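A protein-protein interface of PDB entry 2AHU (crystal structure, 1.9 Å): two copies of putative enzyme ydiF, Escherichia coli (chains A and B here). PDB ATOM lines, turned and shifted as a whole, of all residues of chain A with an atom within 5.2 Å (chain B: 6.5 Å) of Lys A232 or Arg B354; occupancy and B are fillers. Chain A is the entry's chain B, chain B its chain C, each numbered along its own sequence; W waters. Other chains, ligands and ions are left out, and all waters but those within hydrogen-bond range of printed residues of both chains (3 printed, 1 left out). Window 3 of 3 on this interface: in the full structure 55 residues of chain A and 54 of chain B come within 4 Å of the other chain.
OD2 of Asp A192 is in salt-bridge range of NH2 of Arg B354 (2.8 Å).
NH1 of Arg B354 lies within salt-bridge range of OE1 of Glu A194 (3.0 Å).
NZ of Lys A232 lies within salt-bridge range of OD1 of Asp B326, 3.9 Å away.
The backbone carbonyl oxygen of Pro A237 is in hydrogen-bond range of the backbone NH of Ile B356 (3.4 Å).
The side-chain carboxylate (OD1) of Asp A192 sits at hydrogen-bond distance from the backbone NH (N) of Glu A194 (2.9 Å).
The side-chain carboxylate (OD1) of Asp A192 lies within hydrogen-bond range of the backbone NH (N) of Tyr A196, at 3.1 Å.
The backbone NH of Ala A233 is in hydrogen-bond range of the side-chain carboxylate of Asp A192, 3.0 Å away.
OG of Ser A193 sits close to N of Lys A232 (3.5 Å).
O of Ile B337 sits at hydrogen-bond distance from N of Arg B354 (2.8 Å).
The backbone carbonyl oxygen (O) of Ala B355 is in hydrogen-bond range of the backbone NH (N) of Ile B337.
Among the printed residues, pairs that only touch across the chains: Tyr A196 with Arg B354, Pro A237 with Thr B353, Pro A237 with Ala B355, Tyr A196 with Ile B329, Ala A233 with Arg B354, Val A240 with Arg B354, Val A240 with Ala B355, Lys A232 with Arg B354, Pro A237 with Arg B354 and Tyr A196 with Ile B337.
Printed residues of chain B within 4 Å of Asp A192: Arg B354.
Of chain B, only Asp B326 and Arg B354 come within 4 Å of Lys A232.
Thr A234 touches none of the printed residues of chain B.
Printed residues of chain B within 4 Å of Pro A237: Thr B353 (3.4 Å), Arg B354 (3.8 Å), Ala B355 (3.4 Å) and Ile B356 (3.4 Å).
Of the printed residues of chain A, Ile B337 touches Tyr A196.
Gly B338 touches none of the printed residues of chain A.
The nearest printed residue of chain A that does not touch Arg B354 is Thr A234 (6.0 Å).
The nearest printed residue of chain A that does not touch Asp B326 is Glu A194 (4.6 Å).
Printed residues of chain A that touch a printed residue of chain B: Asp A192, Glu A194, Tyr A196, Lys A232, Ala A233, Pro A237 and Val A240.
Along chain A the printed residues that touch a printed residue of chain B span positions 192 to 240.
Among the printed residues, Asp or Glu carboxylates within 4 Å of a Lys or Arg side-chain nitrogen of the other chain: Asp A192 with Arg B354 (2.8 Å), Glu A194 with Arg B354 (3.0 Å) and Lys A232 with Asp B326 (3.9 Å).
No position is printed for both chains.
Of the 14 pairs that touch across the chains among the printed residues, none has its exchanged pair printed and touching as well.
Water W3 lies within hydrogen-bond range of the backbone carbonyl oxygen (O) of Asp B326 (2.6 Å), the side-chain carboxylate (OE2) of Glu A194 (2.9 Å) and the side-chain amino group (NZ) of Lys A232 (3.2 Å).
Water W1 lies within hydrogen-bond range of the side-chain carboxylate of Glu A194, the side-chain hydroxyl of Tyr A196 and the guanidinium group of Arg B354.
Water W2 bridges the side-chain carboxylate (OD1) of Asp B326 (2.8 Å) and the side-chain amino group (NZ) of Lys A232 (3.0 Å).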
ATOM      1  N   ASP A 192      32.654  10.433 -16.170  1.00  0.00           N
ATOM      2  CA  ASP A 192      31.249  10.573 -16.532  1.00  0.00           C
ATOM      3  C   ASP A 192      30.458  11.311 -15.439  1.00  0.00           C
ATOM      4  O   ASP A 192      31.039  11.735 -14.429  1.00  0.00           O
ATOM      5  CB  ASP A 192      30.629   9.236 -17.007  1.00  0.00           C
ATOM      6  CG  ASP A 192      30.268   8.271 -15.875  1.00  0.00           C
ATOM      7  OD1 ASP A 192      30.357   8.643 -14.677  1.00  0.00           O
ATOM      8  OD2 ASP A 192      29.858   7.096 -16.123  1.00  0.00           O
ATOM      9  N   SER A 193      29.154  11.488 -15.653  1.00  0.00           N
ATOM     10  CA  SER A 193      28.316  12.310 -14.767  1.00  0.00           C
ATOM     11  C   SER A 193      28.175  11.714 -13.368  1.00  0.00           C
ATOM     12  O   SER A 193      27.744  12.400 -12.427  1.00  0.00           O
ATOM     13  CB  SER A 193      26.936  12.528 -15.386  1.00  0.00           C
ATOM     14  OG  SER A 193      26.299  11.283 -15.603  1.00  0.00           O
ATOM     15  N   GLU A 194      28.571  10.451 -13.227  1.00  0.00           N
ATOM     16  CA  GLU A 194      28.519   9.775 -11.931  1.00  0.00           C
ATOM     17  C   GLU A 194      29.895   9.610 -11.265  1.00  0.00           C
ATOM     18  O   GLU A 194      30.002   9.010 -10.197  1.00  0.00           O
ATOM     19  CB  GLU A 194      27.822   8.420 -12.072  1.00  0.00           C
ATOM     20  CG  GLU A 194      26.338   8.537 -12.383  1.00  0.00           C
ATOM     21  CD  GLU A 194      25.627   7.208 -12.310  1.00  0.00           C
ATOM     22  OE1 GLU A 194      26.301   6.154 -12.377  1.00  0.00           O
ATOM     23  OE2 GLU A 194      24.388   7.215 -12.181  1.00  0.00           O
ATOM     24  N   TYR A 196      32.755   8.182 -12.720  1.00  0.00           N
ATOM     25  CA  TYR A 196      33.597   7.079 -13.227  1.00  0.00           C
ATOM     26  C   TYR A 196      34.682   7.681 -14.112  1.00  0.00           C
ATOM     27  O   TYR A 196      34.363   8.401 -15.055  1.00  0.00           O
ATOM     28  CB  TYR A 196      32.758   6.045 -13.989  1.00  0.00           C
ATOM     29  CG  TYR A 196      31.896   5.181 -13.091  1.00  0.00           C
ATOM     30  CD1 TYR A 196      30.692   5.667 -12.567  1.00  0.00           C
ATOM     31  CD2 TYR A 196      32.291   3.881 -12.761  1.00  0.00           C
ATOM     32  CE1 TYR A 196      29.897   4.873 -11.732  1.00  0.00           C
ATOM     33  CE2 TYR A 196      31.509   3.079 -11.926  1.00  0.00           C
ATOM     34  CZ  TYR A 196      30.315   3.577 -11.426  1.00  0.00           C
ATOM     35  OH  TYR A 196      29.547   2.787 -10.604  1.00  0.00           O
ATOM     36  N   VAL A 230      31.696  13.659 -19.230  1.00  0.00           N
ATOM     37  CA  VAL A 230      30.988  13.051 -20.352  1.00  0.00           C
ATOM     38  C   VAL A 230      29.696  12.407 -19.853  1.00  0.00           C
ATOM     39  O   VAL A 230      29.488  12.283 -18.642  1.00  0.00           O
ATOM     40  CB  VAL A 230      31.873  11.992 -21.085  1.00  0.00           C
ATOM     41  CG1 VAL A 230      33.200  12.613 -21.560  1.00  0.00           C
ATOM     42  CG2 VAL A 230      32.123  10.747 -20.197  1.00  0.00           C
ATOM     43  N   LYS A 231      28.839  12.002 -20.790  1.00  0.00           N
ATOM     44  CA  LYS A 231      27.572  11.342 -20.462  1.00  0.00           C
ATOM     45  C   LYS A 231      27.774  10.028 -19.704  1.00  0.00           C
ATOM     46  O   LYS A 231      28.678   9.240 -20.022  1.00  0.00           O
ATOM     47  CB  LYS A 231      26.772  11.088 -21.739  1.00  0.00           C
ATOM     48  CG  LYS A 231      25.328  10.604 -21.516  1.00  0.00           C
ATOM     49  CD  LYS A 231      24.693  10.187 -22.841  1.00  0.00           C
ATOM     50  CE  LYS A 231      23.291   9.605 -22.625  1.00  0.00           C
ATOM     51  NZ  LYS A 231      22.676   9.157 -23.925  1.00  0.00           N
ATOM     52  N   LYS A 232      26.927   9.820 -18.696  1.00  0.00           N
ATOM     53  CA  LYS A 232      26.866   8.583 -17.926  1.00  0.00           C
ATOM     54  C   LYS A 232      27.033   7.343 -18.797  1.00  0.00           C
ATOM     55  O   LYS A 232      26.417   7.229 -19.868  1.00  0.00           O
ATOM     56  CB  LYS A 232      25.514   8.512 -17.190  1.00  0.00           C
ATOM     57  CG  LYS A 232      25.292   7.237 -16.403  1.00  0.00           C
ATOM     58  CD  LYS A 232      23.808   7.069 -16.026  1.00  0.00           C
ATOM     59  CE  LYS A 232      23.562   5.653 -15.498  1.00  0.00           C
ATOM     60  NZ  LYS A 232      22.127   5.420 -15.130  1.00  0.00           N
ATOM     61  N   ALA A 233      27.880   6.425 -18.331  1.00  0.00           N
ATOM     62  CA  ALA A 233      28.064   5.108 -18.943  1.00  0.00           C
ATOM     63  C   ALA A 233      28.480   5.116 -20.419  1.00  0.00           C
ATOM     64  O   ALA A 233      28.144   4.195 -21.161  1.00  0.00           O
ATOM     65  CB  ALA A 233      26.809   4.237 -18.732  1.00  0.00           C
ATOM     66  N   THR A 234      29.214   6.139 -20.848  1.00  0.00           N
ATOM     67  CA  THR A 234      29.723   6.161 -22.225  1.00  0.00           C
ATOM     68  C   THR A 234      31.212   5.828 -22.332  1.00  0.00           C
ATOM     69  O   THR A 234      31.725   5.700 -23.431  1.00  0.00           O
ATOM     70  CB  THR A 234      29.430   7.504 -22.939  1.00  0.00           C
ATOM     71  OG1 THR A 234      29.997   8.591 -22.190  1.00  0.00           O
ATOM     72  CG2 THR A 234      27.929   7.782 -22.977  1.00  0.00           C
ATOM     73  N   PRO A 237      34.377   0.340 -20.078  1.00  0.00           N
ATOM     74  CA  PRO A 237      34.571  -0.137 -18.702  1.00  0.00           C
ATOM     75  C   PRO A 237      35.994  -0.598 -18.378  1.00  0.00           C
ATOM     76  O   PRO A 237      36.432  -0.462 -17.237  1.00  0.00           O
ATOM     77  CB  PRO A 237      33.566  -1.294 -18.567  1.00  0.00           C
ATOM     78  CG  PRO A 237      33.212  -1.671 -19.974  1.00  0.00           C
ATOM     79  CD  PRO A 237      33.258  -0.364 -20.739  1.00  0.00           C
ATOM     80  N   VAL A 240      38.123   2.482 -17.386  1.00  0.00           N
ATOM     81  CA  VAL A 240      37.791   3.151 -16.119  1.00  0.00           C
ATOM     82  C   VAL A 240      38.729   2.656 -15.014  1.00  0.00           C
ATOM     83  O   VAL A 240      38.844   1.448 -14.795  1.00  0.00           O
ATOM     84  CB  VAL A 240      36.289   2.969 -15.750  1.00  0.00           C
ATOM     85  CG1 VAL A 240      35.972   3.607 -14.390  1.00  0.00           C
ATOM     86  CG2 VAL A 240      35.393   3.577 -16.829  1.00  0.00           C
ATOM     87  N   ASP B 326      18.884   1.800 -11.652  1.00  0.00           N
ATOM     88  CA  ASP B 326      19.890   2.843 -11.837  1.00  0.00           C
ATOM     89  C   ASP B 326      20.139   3.690 -10.575  1.00  0.00           C
ATOM     90  O   ASP B 326      21.005   4.568 -10.577  1.00  0.00           O
ATOM     91  CB  ASP B 326      19.523   3.736 -13.031  1.00  0.00           C
ATOM     92  CG  ASP B 326      19.324   2.943 -14.320  1.00  0.00           C
ATOM     93  OD1 ASP B 326      20.143   2.044 -14.624  1.00  0.00           O
ATOM     94  OD2 ASP B 326      18.369   3.159 -15.101  1.00  0.00           O
ATOM     95  N   ILE B 329      24.279   0.728  -7.074  1.00  0.00           N
ATOM     96  CA  ILE B 329      25.295   0.036  -7.865  1.00  0.00           C
ATOM     97  C   ILE B 329      25.709  -1.266  -7.183  1.00  0.00           C
ATOM     98  O   ILE B 329      26.025  -1.262  -6.001  1.00  0.00           O
ATOM     99  CB  ILE B 329      26.535   0.964  -8.145  1.00  0.00           C
ATOM    100  CG1 ILE B 329      27.490   0.322  -9.157  1.00  0.00           C
ATOM    101  CG2 ILE B 329      27.299   1.313  -6.862  1.00  0.00           C
ATOM    102  CD1 ILE B 329      26.981   0.317 -10.572  1.00  0.00           C
ATOM    103  N   PRO B 336      34.228  -6.942 -11.510  1.00  0.00           N
ATOM    104  CA  PRO B 336      33.223  -6.166 -12.249  1.00  0.00           C
ATOM    105  C   PRO B 336      32.354  -5.266 -11.389  1.00  0.00           C
ATOM    106  O   PRO B 336      31.934  -5.653 -10.287  1.00  0.00           O
ATOM    107  CB  PRO B 336      32.375  -7.246 -12.926  1.00  0.00           C
ATOM    108  CG  PRO B 336      33.336  -8.397 -13.056  1.00  0.00           C
ATOM    109  CD  PRO B 336      34.059  -8.389 -11.733  1.00  0.00           C
ATOM    110  N   ILE B 337      32.100  -4.062 -11.900  1.00  0.00           N
ATOM    111  CA  ILE B 337      31.237  -3.110 -11.230  1.00  0.00           C
ATOM    112  C   ILE B 337      30.059  -2.795 -12.157  1.00  0.00           C
ATOM    113  O   ILE B 337      30.256  -2.317 -13.282  1.00  0.00           O
ATOM    114  CB  ILE B 337      32.035  -1.835 -10.854  1.00  0.00           C
ATOM    115  CG1 ILE B 337      33.142  -2.194  -9.844  1.00  0.00           C
ATOM    116  CG2 ILE B 337      31.099  -0.760 -10.278  1.00  0.00           C
ATOM    117  CD1 ILE B 337      34.294  -1.194  -9.807  1.00  0.00           C
ATOM    118  N   GLY B 338      28.848  -3.106 -11.695  1.00  0.00           N
ATOM    119  CA  GLY B 338      27.645  -2.775 -12.445  1.00  0.00           C
ATOM    120  C   GLY B 338      27.385  -3.784 -13.549  1.00  0.00           C
ATOM    121  O   GLY B 338      28.045  -4.817 -13.633  1.00  0.00           O
ATOM    122  N   GLY B 339      26.422  -3.485 -14.406  1.00  0.00           N
ATOM    123  CA  GLY B 339      26.108  -4.382 -15.513  1.00  0.00           C
ATOM    124  C   GLY B 339      24.755  -5.041 -15.324  1.00  0.00           C
ATOM    125  O   GLY B 339      24.129  -4.906 -14.266  1.00  0.00           O
ATOM    126  N   VAL B 351      26.804  -7.879 -18.929  1.00  0.00           N
ATOM    127  CA  VAL B 351      27.192  -6.911 -19.952  1.00  0.00           C
ATOM    128  C   VAL B 351      26.861  -5.503 -19.467  1.00  0.00           C
ATOM    129  O   VAL B 351      26.228  -5.343 -18.423  1.00  0.00           O
ATOM    130  CB  VAL B 351      26.511  -7.188 -21.310  1.00  0.00           C
ATOM    131  CG1 VAL B 351      26.948  -8.556 -21.837  1.00  0.00           C
ATOM    132  CG2 VAL B 351      24.985  -7.115 -21.189  1.00  0.00           C
ATOM    133  N   ASN B 352      27.301  -4.499 -20.228  1.00  0.00           N
ATOM    134  CA  ASN B 352      27.111  -3.090 -19.873  1.00  0.00           C
ATOM    135  C   ASN B 352      27.681  -2.772 -18.488  1.00  0.00           C
ATOM    136  O   ASN B 352      27.107  -1.970 -17.750  1.00  0.00           O
ATOM    137  CB  ASN B 352      25.628  -2.683 -19.928  1.00  0.00           C
ATOM    138  CG  ASN B 352      25.022  -2.787 -21.316  1.00  0.00           C
ATOM    139  OD1 ASN B 352      25.701  -3.127 -22.288  1.00  0.00           O
ATOM    140  ND2 ASN B 352      23.723  -2.490 -21.417  1.00  0.00           N
ATOM    141  N   THR B 353      28.801  -3.403 -18.134  1.00  0.00           N
ATOM    142  CA  THR B 353      29.482  -3.082 -16.873  1.00  0.00           C
ATOM    143  C   THR B 353      29.996  -1.646 -16.907  1.00  0.00           C
ATOM    144  O   THR B 353      30.217  -1.079 -17.986  1.00  0.00           O
ATOM    145  CB  THR B 353      30.631  -4.071 -16.562  1.00  0.00           C
ATOM    146  OG1 THR B 353      31.679  -3.927 -17.536  1.00  0.00           O
ATOM    147  CG2 THR B 353      30.156  -5.506 -16.735  1.00  0.00           C
ATOM    148  N   ARG B 354      30.185  -1.064 -15.729  1.00  0.00           N
ATOM    149  CA  ARG B 354      30.632   0.321 -15.622  1.00  0.00           C
ATOM    150  C   ARG B 354      32.137   0.421 -15.430  1.00  0.00           C
ATOM    151  O   ARG B 354      32.736   1.446 -15.742  1.00  0.00           O
ATOM    152  CB  ARG B 354      29.906   1.035 -14.482  1.00  0.00           C
ATOM    153  CG  ARG B 354      28.383   1.078 -14.635  1.00  0.00           C
ATOM    154  CD  ARG B 354      27.897   1.966 -15.809  1.00  0.00           C
ATOM    155  NE  ARG B 354      28.316   3.355 -15.614  1.00  0.00           N
ATOM    156  CZ  ARG B 354      27.675   4.213 -14.830  1.00  0.00           C
ATOM    157  NH1 ARG B 354      26.579   3.831 -14.178  1.00  0.00           N
ATOM    158  NH2 ARG B 354      28.128   5.454 -14.692  1.00  0.00           N
ATOM    159  N   ALA B 355      32.739  -0.647 -14.904  1.00  0.00           N
ATOM    160  CA  ALA B 355      34.177  -0.700 -14.669  1.00  0.00           C
ATOM    161  C   ALA B 355      34.546  -2.123 -14.309  1.00  0.00           C
ATOM    162  O   ALA B 355      33.692  -2.892 -13.869  1.00  0.00           O
ATOM    163  CB  ALA B 355      34.573   0.238 -13.527  1.00  0.00           C
ATOM    164  N   ILE B 356      35.818  -2.464 -14.506  1.00  0.00           N
ATOM    165  CA  ILE B 356      36.363  -3.734 -14.031  1.00  0.00           C
ATOM    166  C   ILE B 356      37.653  -3.462 -13.268  1.00  0.00           C
ATOM    167  O   ILE B 356      38.640  -3.010 -13.858  1.00  0.00           O
ATOM    168  CB  ILE B 356      36.609  -4.717 -15.199  1.00  0.00           C
ATOM    169  CG1 ILE B 356      35.321  -4.932 -16.001  1.00  0.00           C
ATOM    170  CG2 ILE B 356      37.152  -6.072 -14.648  1.00  0.00           C
ATOM    171  CD1 ILE B 356      35.497  -5.685 -17.291  1.00  0.00           C
HETATM  172  O   HOH W   1      26.840   3.881 -10.866  1.00  0.00           O
HETATM  173  O   HOH W   2      22.890   2.626 -14.276  1.00  0.00           O
HETATM  174  O   HOH W   3      23.082   4.651 -12.155  1.00  0.00           O
